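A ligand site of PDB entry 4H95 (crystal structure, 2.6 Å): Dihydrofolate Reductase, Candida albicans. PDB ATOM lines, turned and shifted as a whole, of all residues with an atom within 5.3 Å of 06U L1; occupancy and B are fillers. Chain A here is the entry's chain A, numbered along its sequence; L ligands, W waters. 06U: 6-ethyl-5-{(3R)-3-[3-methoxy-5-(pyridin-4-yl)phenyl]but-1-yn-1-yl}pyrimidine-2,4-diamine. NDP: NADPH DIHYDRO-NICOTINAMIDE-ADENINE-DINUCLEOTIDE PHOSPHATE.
The side-chain hydroxyl (OG1) of Thr 130 is in hydrogen-bond range of the side-chain carboxylate (OE2) of Glu 29 (2.8 Å).
The side-chain hydroxyl (OH) of Tyr 115 sits at hydrogen-bond distance from the backbone carbonyl oxygen (O) of Ile 109.
The side-chain hydroxyl (OH) of Tyr 115 lies within hydrogen-bond range of the backbone carbonyl oxygen (O) of Ile 6, at 2.8 Å.
The side-chain hydroxyl (OH) of Tyr 115 lies within hydrogen-bond range of the backbone NH (N) of Gly 110, at 3.4 Å.
The backbone NH (N) of Ile 6 lies within hydrogen-bond range of the backbone carbonyl oxygen (O) of Ile 108, at 3.0 Å.
The side-chain hydroxyl (OG) of Ser 58 sits at hydrogen-bond distance from the backbone carbonyl oxygen (O) of Thr 55 (2.6 Å).
The backbone NH of Thr 130 is in hydrogen-bond range of the backbone carbonyl oxygen of Val 7 (2.9 Å).
The backbone carbonyl oxygen (O) of Leu 128 is in hydrogen-bond range of the backbone NH (N) of Val 7, at 2.9 Å.
O7N of NDP L2 sits close to NAJ of 06U L1.
Water W2 lies within hydrogen-bond range of OG1 of Thr 130 (2.7 Å), O of Leu 128 (2.9 Å), O of Val 7 (3.2 Å) and NAH of 06U L1 (3.4 Å).
The backbone carbonyl oxygen of Ser 58 sits close to an oxygen (OBA) of 06U L1.
Residues that only touch 06U L1: Val 7, Met 22, Phe 33, Pro 60, Ile 30, Thr 55, Ala 8, Thr 130 and Leu 66.
14 residues have an atom within 4 Å of 06U L1: Ile 6, Val 7, Ala 8, Met 22, Glu 29, Ile 30, Phe 33, Thr 55, Ser 58, Pro 60, Leu 66, Ile 109, Tyr 115 and Thr 130.
The nearest printed residue that does not touch 06U L1 is Phe 63 (4.05 Å).
The side-chain carboxylate (OE2) of Glu 29 sits at hydrogen-bond distance from a nitrogen (NAH) of 06U L1 (2.6 Å).
O of Ile 109 is in hydrogen-bond range of NAJ of 06U L1 (2.9 Å).
The side-chain hydroxyl of Tyr 115 is in hydrogen-bond range of a nitrogen (NAJ) of 06U L1, 2.9 Å away.
The backbone carbonyl oxygen (O) of Ile 6 is in hydrogen-bond range of a nitrogen (NAJ) of 06U L1.
The backbone NH (N) of Met 22 is in hydrogen-bond range of an oxygen (O2D) of NDP L2 (3.4 Å).
The backbone NH (N) of Thr 55 sits close to an oxygen (O2A) of NDP L2, at 3.4 Å.
OG1 of Thr 55 sits at hydrogen-bond distance from O2A of NDP L2 (2.5 Å).
The backbone NH (N) of Ala 8 lies within hydrogen-bond range of an oxygen (O7N) of NDP L2, 3.0 Å away.
A nitrogen (N7N) of NDP L2 lies within hydrogen-bond range of the backbone carbonyl oxygen of Ala 8, 2.7 Å away.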
ATOM      1  N   ILE A   6      -5.962 -25.496  11.725  1.00  0.00           N
ATOM      2  CA  ILE A   6      -4.945 -24.678  11.070  1.00  0.00           C
ATOM      3  C   ILE A   6      -4.434 -23.601  12.030  1.00  0.00           C
ATOM      4  O   ILE A   6      -5.221 -22.827  12.596  1.00  0.00           O
ATOM      5  CB  ILE A   6      -5.463 -24.087   9.715  1.00  0.00           C
ATOM      6  CG1 ILE A   6      -4.345 -23.331   8.976  1.00  0.00           C
ATOM      7  CG2 ILE A   6      -6.718 -23.238   9.915  1.00  0.00           C
ATOM      8  CD1 ILE A   6      -4.610 -23.126   7.492  1.00  0.00           C
ATOM      9  N   VAL A   7      -3.122 -23.569  12.215  1.00  0.00           N
ATOM     10  CA  VAL A   7      -2.482 -22.700  13.214  1.00  0.00           C
ATOM     11  C   VAL A   7      -1.014 -22.424  12.852  1.00  0.00           C
ATOM     12  O   VAL A   7      -0.373 -23.221  12.175  1.00  0.00           O
ATOM     13  CB  VAL A   7      -2.574 -23.318  14.641  1.00  0.00           C
ATOM     14  CG1 VAL A   7      -1.837 -24.668  14.727  1.00  0.00           C
ATOM     15  CG2 VAL A   7      -2.078 -22.340  15.713  1.00  0.00           C
ATOM     16  N   ALA A   8      -0.508 -21.269  13.294  1.00  0.00           N
ATOM     17  CA  ALA A   8       0.913 -20.944  13.210  1.00  0.00           C
ATOM     18  C   ALA A   8       1.494 -20.743  14.610  1.00  0.00           C
ATOM     19  O   ALA A   8       1.028 -19.890  15.366  1.00  0.00           O
ATOM     20  CB  ALA A   8       1.131 -19.712  12.352  1.00  0.00           C
ATOM     21  N   MET A  22      -1.206 -11.616  18.348  1.00  0.00           N
ATOM     22  CA  MET A  22      -0.169 -12.395  17.669  1.00  0.00           C
ATOM     23  C   MET A  22       1.190 -11.689  17.707  1.00  0.00           C
ATOM     24  O   MET A  22       1.263 -10.486  17.453  1.00  0.00           O
ATOM     25  CB  MET A  22      -0.586 -12.674  16.232  1.00  0.00           C
ATOM     26  CG  MET A  22      -1.900 -13.437  16.096  1.00  0.00           C
ATOM     27  SD  MET A  22      -2.247 -14.020  14.423  1.00  0.00           S
ATOM     28  CE  MET A  22      -0.968 -15.258  14.226  1.00  0.00           C
ATOM     29  N   GLU A  29       2.373 -16.093   5.114  1.00  0.00           N
ATOM     30  CA  GLU A  29       1.608 -17.006   5.962  1.00  0.00           C
ATOM     31  C   GLU A  29       0.114 -16.665   5.917  1.00  0.00           C
ATOM     32  O   GLU A  29      -0.727 -17.562   5.863  1.00  0.00           O
ATOM     33  CB  GLU A  29       2.126 -16.952   7.402  1.00  0.00           C
ATOM     34  CG  GLU A  29       2.002 -18.257   8.178  1.00  0.00           C
ATOM     35  CD  GLU A  29       0.570 -18.606   8.535  1.00  0.00           C
ATOM     36  OE1 GLU A  29      -0.194 -17.700   8.934  1.00  0.00           O
ATOM     37  OE2 GLU A  29       0.206 -19.796   8.424  1.00  0.00           O
ATOM     38  N   ILE A  30      -0.193 -15.362   5.933  1.00  0.00           N
ATOM     39  CA  ILE A  30      -1.568 -14.865   5.853  1.00  0.00           C
ATOM     40  C   ILE A  30      -2.262 -15.287   4.545  1.00  0.00           C
ATOM     41  O   ILE A  30      -3.412 -15.711   4.563  1.00  0.00           O
ATOM     42  CB  ILE A  30      -1.626 -13.317   6.048  1.00  0.00           C
ATOM     43  CG1 ILE A  30      -1.373 -12.967   7.519  1.00  0.00           C
ATOM     44  CG2 ILE A  30      -2.966 -12.743   5.588  1.00  0.00           C
ATOM     45  CD1 ILE A  30      -0.879 -11.543   7.749  1.00  0.00           C
ATOM     46  N   TYR A  32      -1.373 -17.856   2.656  1.00  0.00           N
ATOM     47  CA  TYR A  32      -1.498 -19.316   2.745  1.00  0.00           C
ATOM     48  C   TYR A  32      -2.767 -19.704   3.500  1.00  0.00           C
ATOM     49  O   TYR A  32      -3.530 -20.564   3.036  1.00  0.00           O
ATOM     50  CB  TYR A  32      -0.261 -19.915   3.422  1.00  0.00           C
ATOM     51  CG  TYR A  32      -0.368 -21.396   3.724  1.00  0.00           C
ATOM     52  CD1 TYR A  32      -0.031 -22.338   2.755  1.00  0.00           C
ATOM     53  CD2 TYR A  32      -0.790 -21.852   4.975  1.00  0.00           C
ATOM     54  CE1 TYR A  32      -0.124 -23.695   3.016  1.00  0.00           C
ATOM     55  CE2 TYR A  32      -0.890 -23.202   5.246  1.00  0.00           C
ATOM     56  CZ  TYR A  32      -0.547 -24.117   4.265  1.00  0.00           C
ATOM     57  OH  TYR A  32      -0.633 -25.471   4.520  1.00  0.00           O
ATOM     58  N   PHE A  33      -2.977 -19.070   4.651  1.00  0.00           N
ATOM     59  CA  PHE A  33      -4.192 -19.256   5.442  1.00  0.00           C
ATOM     60  C   PHE A  33      -5.431 -18.964   4.588  1.00  0.00           C
ATOM     61  O   PHE A  33      -6.402 -19.714   4.622  1.00  0.00           O
ATOM     62  CB  PHE A  33      -4.158 -18.338   6.673  1.00  0.00           C
ATOM     63  CG  PHE A  33      -5.446 -18.288   7.436  1.00  0.00           C
ATOM     64  CD1 PHE A  33      -5.739 -19.251   8.401  1.00  0.00           C
ATOM     65  CD2 PHE A  33      -6.369 -17.271   7.206  1.00  0.00           C
ATOM     66  CE1 PHE A  33      -6.933 -19.209   9.109  1.00  0.00           C
ATOM     67  CE2 PHE A  33      -7.563 -17.220   7.918  1.00  0.00           C
ATOM     68  CZ  PHE A  33      -7.842 -18.202   8.875  1.00  0.00           C
ATOM     69  N   THR A  55     -11.667 -14.727  19.363  1.00  0.00           N
ATOM     70  CA  THR A  55     -10.965 -14.676  18.083  1.00  0.00           C
ATOM     71  C   THR A  55     -11.773 -13.898  17.057  1.00  0.00           C
ATOM     72  O   THR A  55     -11.236 -13.054  16.346  1.00  0.00           O
ATOM     73  CB  THR A  55     -10.641 -16.107  17.581  1.00  0.00           C
ATOM     74  OG1 THR A  55      -9.740 -16.736  18.508  1.00  0.00           O
ATOM     75  CG2 THR A  55      -9.993 -16.071  16.202  1.00  0.00           C
ATOM     76  N   SER A  58     -11.421 -10.324  17.563  1.00  0.00           N
ATOM     77  CA  SER A  58     -10.070  -9.846  17.311  1.00  0.00           C
ATOM     78  C   SER A  58      -9.797  -9.571  15.833  1.00  0.00           C
ATOM     79  O   SER A  58      -8.856  -8.847  15.490  1.00  0.00           O
ATOM     80  CB  SER A  58      -9.025 -10.818  17.865  1.00  0.00           C
ATOM     81  OG  SER A  58      -8.974 -12.022  17.107  1.00  0.00           O
ATOM     82  N   ILE A  59     -10.625 -10.135  14.953  1.00  0.00           N
ATOM     83  CA  ILE A  59     -10.473  -9.940  13.509  1.00  0.00           C
ATOM     84  C   ILE A  59     -10.810  -8.500  13.131  1.00  0.00           C
ATOM     85  O   ILE A  59     -11.827  -7.970  13.572  1.00  0.00           O
ATOM     86  CB  ILE A  59     -11.349 -10.944  12.703  1.00  0.00           C
ATOM     87  CG1 ILE A  59     -10.955 -12.387  13.035  1.00  0.00           C
ATOM     88  CG2 ILE A  59     -11.203 -10.702  11.194  1.00  0.00           C
ATOM     89  CD1 ILE A  59     -11.963 -13.416  12.553  1.00  0.00           C
ATOM     90  N   PRO A  60      -9.938  -7.858  12.319  1.00  0.00           N
ATOM     91  CA  PRO A  60     -10.194  -6.496  11.842  1.00  0.00           C
ATOM     92  C   PRO A  60     -11.607  -6.326  11.287  1.00  0.00           C
ATOM     93  O   PRO A  60     -12.111  -7.216  10.586  1.00  0.00           O
ATOM     94  CB  PRO A  60      -9.157  -6.321  10.724  1.00  0.00           C
ATOM     95  CG  PRO A  60      -8.013  -7.166  11.179  1.00  0.00           C
ATOM     96  CD  PRO A  60      -8.597  -8.335  11.919  1.00  0.00           C
ATOM     97  N   PHE A  63     -12.420  -7.191   7.778  1.00  0.00           N
ATOM     98  CA  PHE A  63     -12.049  -8.564   7.400  1.00  0.00           C
ATOM     99  C   PHE A  63     -13.047  -9.611   7.901  1.00  0.00           C
ATOM    100  O   PHE A  63     -12.946 -10.783   7.522  1.00  0.00           O
ATOM    101  CB  PHE A  63     -10.634  -8.900   7.888  1.00  0.00           C
ATOM    102  CG  PHE A  63      -9.533  -8.358   7.009  1.00  0.00           C
ATOM    103  CD1 PHE A  63      -9.663  -8.371   5.615  1.00  0.00           C
ATOM    104  CD2 PHE A  63      -8.359  -7.877   7.572  1.00  0.00           C
ATOM    105  CE1 PHE A  63      -8.641  -7.877   4.800  1.00  0.00           C
ATOM    106  CE2 PHE A  63      -7.330  -7.376   6.767  1.00  0.00           C
ATOM    107  CZ  PHE A  63      -7.481  -7.382   5.383  1.00  0.00           C
ATOM    108  N   LEU A  66     -15.029 -13.467   7.311  1.00  0.00           N
ATOM    109  CA  LEU A  66     -14.025 -13.824   6.306  1.00  0.00           C
ATOM    110  C   LEU A  66     -14.727 -14.259   5.030  1.00  0.00           C
ATOM    111  O   LEU A  66     -15.476 -15.240   5.028  1.00  0.00           O
ATOM    112  CB  LEU A  66     -13.078 -14.904   6.830  1.00  0.00           C
ATOM    113  CG  LEU A  66     -12.255 -14.602   8.093  1.00  0.00           C
ATOM    114  CD1 LEU A  66     -11.697 -15.880   8.692  1.00  0.00           C
ATOM    115  CD2 LEU A  66     -11.133 -13.601   7.818  1.00  0.00           C
ATOM    116  N   ILE A 108     -10.543 -25.209  11.885  1.00  0.00           N
ATOM    117  CA  ILE A 108     -10.480 -24.583  13.198  1.00  0.00           C
ATOM    118  C   ILE A 108      -9.356 -23.557  13.155  1.00  0.00           C
ATOM    119  O   ILE A 108      -8.182 -23.908  12.947  1.00  0.00           O
ATOM    120  CB  ILE A 108     -10.217 -25.621  14.316  1.00  0.00           C
ATOM    121  CG1 ILE A 108     -11.145 -26.843  14.184  1.00  0.00           C
ATOM    122  CG2 ILE A 108     -10.311 -24.971  15.697  1.00  0.00           C
ATOM    123  CD1 ILE A 108     -12.633 -26.530  14.181  1.00  0.00           C
ATOM    124  N   ILE A 109      -9.709 -22.294  13.352  1.00  0.00           N
ATOM    125  CA  ILE A 109      -8.766 -21.196  13.123  1.00  0.00           C
ATOM    126  C   ILE A 109      -8.406 -20.395  14.388  1.00  0.00           C
ATOM    127  O   ILE A 109      -7.705 -19.389  14.300  1.00  0.00           O
ATOM    128  CB  ILE A 109      -9.247 -20.250  11.986  1.00  0.00           C
ATOM    129  CG1 ILE A 109     -10.485 -19.451  12.419  1.00  0.00           C
ATOM    130  CG2 ILE A 109      -9.522 -21.045  10.710  1.00  0.00           C
ATOM    131  CD1 ILE A 109     -10.824 -18.308  11.494  1.00  0.00           C
ATOM    132  N   GLY A 110      -8.862 -20.868  15.547  1.00  0.00           N
ATOM    133  CA  GLY A 110      -8.522 -20.211  16.823  1.00  0.00           C
ATOM    134  C   GLY A 110      -9.694 -20.043  17.780  1.00  0.00           C
ATOM    135  O   GLY A 110     -10.838 -20.280  17.416  1.00  0.00           O
ATOM    136  N   TYR A 115      -8.432 -24.380  20.277  1.00  0.00           N
ATOM    137  CA  TYR A 115      -7.364 -25.305  19.883  1.00  0.00           C
ATOM    138  C   TYR A 115      -7.155 -26.406  20.914  1.00  0.00           C
ATOM    139  O   TYR A 115      -7.267 -27.592  20.588  1.00  0.00           O
ATOM    140  CB  TYR A 115      -6.037 -24.558  19.685  1.00  0.00           C
ATOM    141  CG  TYR A 115      -5.936 -23.725  18.421  1.00  0.00           C
ATOM    142  CD1 TYR A 115      -6.362 -24.214  17.181  1.00  0.00           C
ATOM    143  CD2 TYR A 115      -5.359 -22.450  18.462  1.00  0.00           C
ATOM    144  CE1 TYR A 115      -6.248 -23.447  16.028  1.00  0.00           C
ATOM    145  CE2 TYR A 115      -5.245 -21.674  17.313  1.00  0.00           C
ATOM    146  CZ  TYR A 115      -5.686 -22.173  16.099  1.00  0.00           C
ATOM    147  OH  TYR A 115      -5.572 -21.411  14.959  1.00  0.00           O
ATOM    148  N   LEU A 128      -2.831 -28.589  10.421  1.00  0.00           N
ATOM    149  CA  LEU A 128      -2.029 -27.765   9.529  1.00  0.00           C
ATOM    150  C   LEU A 128      -1.239 -26.797  10.395  1.00  0.00           C
ATOM    151  O   LEU A 128      -1.749 -25.748  10.795  1.00  0.00           O
ATOM    152  CB  LEU A 128      -2.922 -27.023   8.534  1.00  0.00           C
ATOM    153  CG  LEU A 128      -3.617 -27.875   7.464  1.00  0.00           C
ATOM    154  CD1 LEU A 128      -4.944 -27.270   7.062  1.00  0.00           C
ATOM    155  CD2 LEU A 128      -2.723 -28.058   6.237  1.00  0.00           C
ATOM    156  N   THR A 130       1.847 -24.338  10.776  1.00  0.00           N
ATOM    157  CA  THR A 130       2.966 -23.530  10.310  1.00  0.00           C
ATOM    158  C   THR A 130       3.970 -23.408  11.464  1.00  0.00           C
ATOM    159  O   THR A 130       3.742 -22.645  12.400  1.00  0.00           O
ATOM    160  CB  THR A 130       2.533 -22.142   9.817  1.00  0.00           C
ATOM    161  OG1 THR A 130       1.549 -22.281   8.786  1.00  0.00           O
ATOM    162  CG2 THR A 130       3.732 -21.384   9.264  1.00  0.00           C
HETATM  163  N1  06U L   1      -3.576 -20.183  11.230  1.00  0.00           N
HETATM  164  C2  06U L   1      -2.608 -19.752  10.328  1.00  0.00           C
HETATM  165  N3  06U L   1      -2.521 -18.400   9.997  1.00  0.00           N
HETATM  166  C4  06U L   1      -3.408 -17.461  10.551  1.00  0.00           C
HETATM  167  C5  06U L   1      -4.376 -17.911  11.446  1.00  0.00           C
HETATM  168  C6  06U L   1      -4.464 -19.260  11.794  1.00  0.00           C
HETATM  169  CAA 06U L   1      -7.529 -12.389   8.612  1.00  0.00           C
HETATM  170  NAH 06U L   1      -1.771 -20.638   9.801  1.00  0.00           N
HETATM  171  CAI 06U L   1      -3.263 -15.991  10.116  1.00  0.00           C
HETATM  172  NAJ 06U L   1      -5.381 -19.690  12.643  1.00  0.00           N
HETATM  173  CAK 06U L   1      -5.292 -16.989  12.039  1.00  0.00           C
HETATM  174  CAL 06U L   1      -6.071 -16.195  12.530  1.00  0.00           C
HETATM  175  CAM 06U L   1      -7.023 -15.272  13.146  1.00  0.00           C
HETATM  176  CAN 06U L   1      -8.442 -15.732  12.818  1.00  0.00           C
HETATM  177  CAO 06U L   1      -6.799 -13.832  12.631  1.00  0.00           C
HETATM  178  CAP 06U L   1      -6.654 -12.804  13.565  1.00  0.00           C
HETATM  179  CAQ 06U L   1      -6.444 -11.487  13.138  1.00  0.00           C
HETATM  180  CAR 06U L   1      -6.408 -11.207  11.772  1.00  0.00           C
HETATM  181  CAS 06U L   1      -6.552 -12.229  10.825  1.00  0.00           C
HETATM  182  CAT 06U L   1      -6.748 -13.543  11.269  1.00  0.00           C
HETATM  183  CAU 06U L   1      -6.515 -11.940   9.463  1.00  0.00           C
HETATM  184  CAV 06U L   1      -5.472 -11.188   8.920  1.00  0.00           C
HETATM  185  CAW 06U L   1      -5.484 -10.915   7.543  1.00  0.00           C
HETATM  186  NAX 06U L   1      -6.464 -11.365   6.776  1.00  0.00           N
HETATM  187  CAY 06U L   1      -7.471 -12.078   7.251  1.00  0.00           C
HETATM  188  CAZ 06U L   1      -2.158 -15.265  10.874  1.00  0.00           C
HETATM  189  OBA 06U L   1      -6.306 -10.470  14.045  1.00  0.00           O
HETATM  190  CBB 06U L   1      -4.973 -10.344  14.588  1.00  0.00           C
HETATM  191  PA  NDP L   2     -10.711 -18.077  21.887  1.00  0.00           P
HETATM  192  O1A NDP L   2     -10.287 -19.473  22.132  1.00  0.00           O
HETATM  193  O2A NDP L   2     -10.934 -17.845  20.444  1.00  0.00           O
HETATM  194  O5B NDP L   2     -12.023 -17.678  22.721  1.00  0.00           O
HETATM  195  C5B NDP L   2     -12.503 -18.459  23.787  1.00  0.00           C
HETATM  196  C4B NDP L   2     -14.018 -18.331  23.816  1.00  0.00           C
HETATM  197  O4B NDP L   2     -14.618 -19.296  22.976  1.00  0.00           O
HETATM  198  C3B NDP L   2     -14.601 -18.553  25.204  1.00  0.00           C
HETATM  199  O3B NDP L   2     -14.729 -17.336  25.898  1.00  0.00           O
HETATM  200  C2B NDP L   2     -15.949 -19.171  24.920  1.00  0.00           C
HETATM  201  O2B NDP L   2     -16.893 -18.154  24.713  1.00  0.00           O
HETATM  202  C1B NDP L   2     -15.749 -19.882  23.585  1.00  0.00           C
HETATM  203  N9A NDP L   2     -15.514 -21.326  23.754  1.00  0.00           N
HETATM  204  C8A NDP L   2     -14.372 -21.926  24.216  1.00  0.00           C
HETATM  205  N7A NDP L   2     -14.539 -23.265  24.216  1.00  0.00           N
HETATM  206  C5A NDP L   2     -15.780 -23.541  23.759  1.00  0.00           C
HETATM  207  C6A NDP L   2     -16.460 -24.742  23.555  1.00  0.00           C
HETATM  208  N6A NDP L   2     -15.869 -25.902  23.836  1.00  0.00           N
HETATM  209  N1A NDP L   2     -17.753 -24.728  23.069  1.00  0.00           N
HETATM  210  C2A NDP L   2     -18.365 -23.517  22.769  1.00  0.00           C
HETATM  211  N3A NDP L   2     -17.678 -22.328  22.976  1.00  0.00           N
HETATM  212  C4A NDP L   2     -16.406 -22.331  23.459  1.00  0.00           C
HETATM  213  O3  NDP L   2      -9.604 -17.055  22.444  1.00  0.00           O
HETATM  214  PN  NDP L   2      -8.370 -17.241  23.463  1.00  0.00           P
HETATM  215  O1N NDP L   2      -8.267 -15.995  24.255  1.00  0.00           O
HETATM  216  O2N NDP L   2      -8.485 -18.540  24.143  1.00  0.00           O
HETATM  217  O5D NDP L   2      -7.113 -17.331  22.447  1.00  0.00           O
HETATM  218  C5D NDP L   2      -6.781 -16.236  21.612  1.00  0.00           C
HETATM  219  C4D NDP L   2      -5.266 -16.128  21.480  1.00  0.00           C
HETATM  220  O4D NDP L   2      -4.795 -17.062  20.524  1.00  0.00           O
HETATM  221  C3D NDP L   2      -4.823 -14.753  21.026  1.00  0.00           C
HETATM  222  O3D NDP L   2      -3.824 -14.281  21.902  1.00  0.00           O
HETATM  223  C2D NDP L   2      -4.244 -14.939  19.634  1.00  0.00           C
HETATM  224  O2D NDP L   2      -3.037 -14.230  19.472  1.00  0.00           O
HETATM  225  C1D NDP L   2      -3.997 -16.435  19.531  1.00  0.00           C
HETATM  226  N1N NDP L   2      -4.287 -16.963  18.178  1.00  0.00           N
HETATM  227  C2N NDP L   2      -3.251 -17.426  17.413  1.00  0.00           C
HETATM  228  C3N NDP L   2      -3.478 -17.940  16.136  1.00  0.00           C
HETATM  229  C7N NDP L   2      -2.341 -18.490  15.322  1.00  0.00           C
HETATM  230  O7N NDP L   2      -2.612 -19.294  14.201  1.00  0.00           O
HETATM  231  N7N NDP L   2      -1.077 -18.225  15.676  1.00  0.00           N
HETATM  232  C4N NDP L   2      -4.777 -17.965  15.641  1.00  0.00           C
HETATM  233  C5N NDP L   2      -5.835 -17.496  16.416  1.00  0.00           C
HETATM  234  C6N NDP L   2      -5.572 -16.993  17.697  1.00  0.00           C
HETATM  235  P2B NDP L   2     -17.978 -17.695  25.811  1.00  0.00           P
HETATM  236  O1X NDP L   2     -18.949 -16.754  25.123  1.00  0.00           O
HETATM  237  O2X NDP L   2     -18.728 -18.886  26.357  1.00  0.00           O
HETATM  238  O3X NDP L   2     -17.283 -16.963  26.939  1.00  0.00           O
HETATM  239  O   HOH W   1       1.006 -16.266  10.748  1.00  0.00           O
HETATM  240  O   HOH W   2      -0.680 -23.722   9.042  1.00  0.00           O
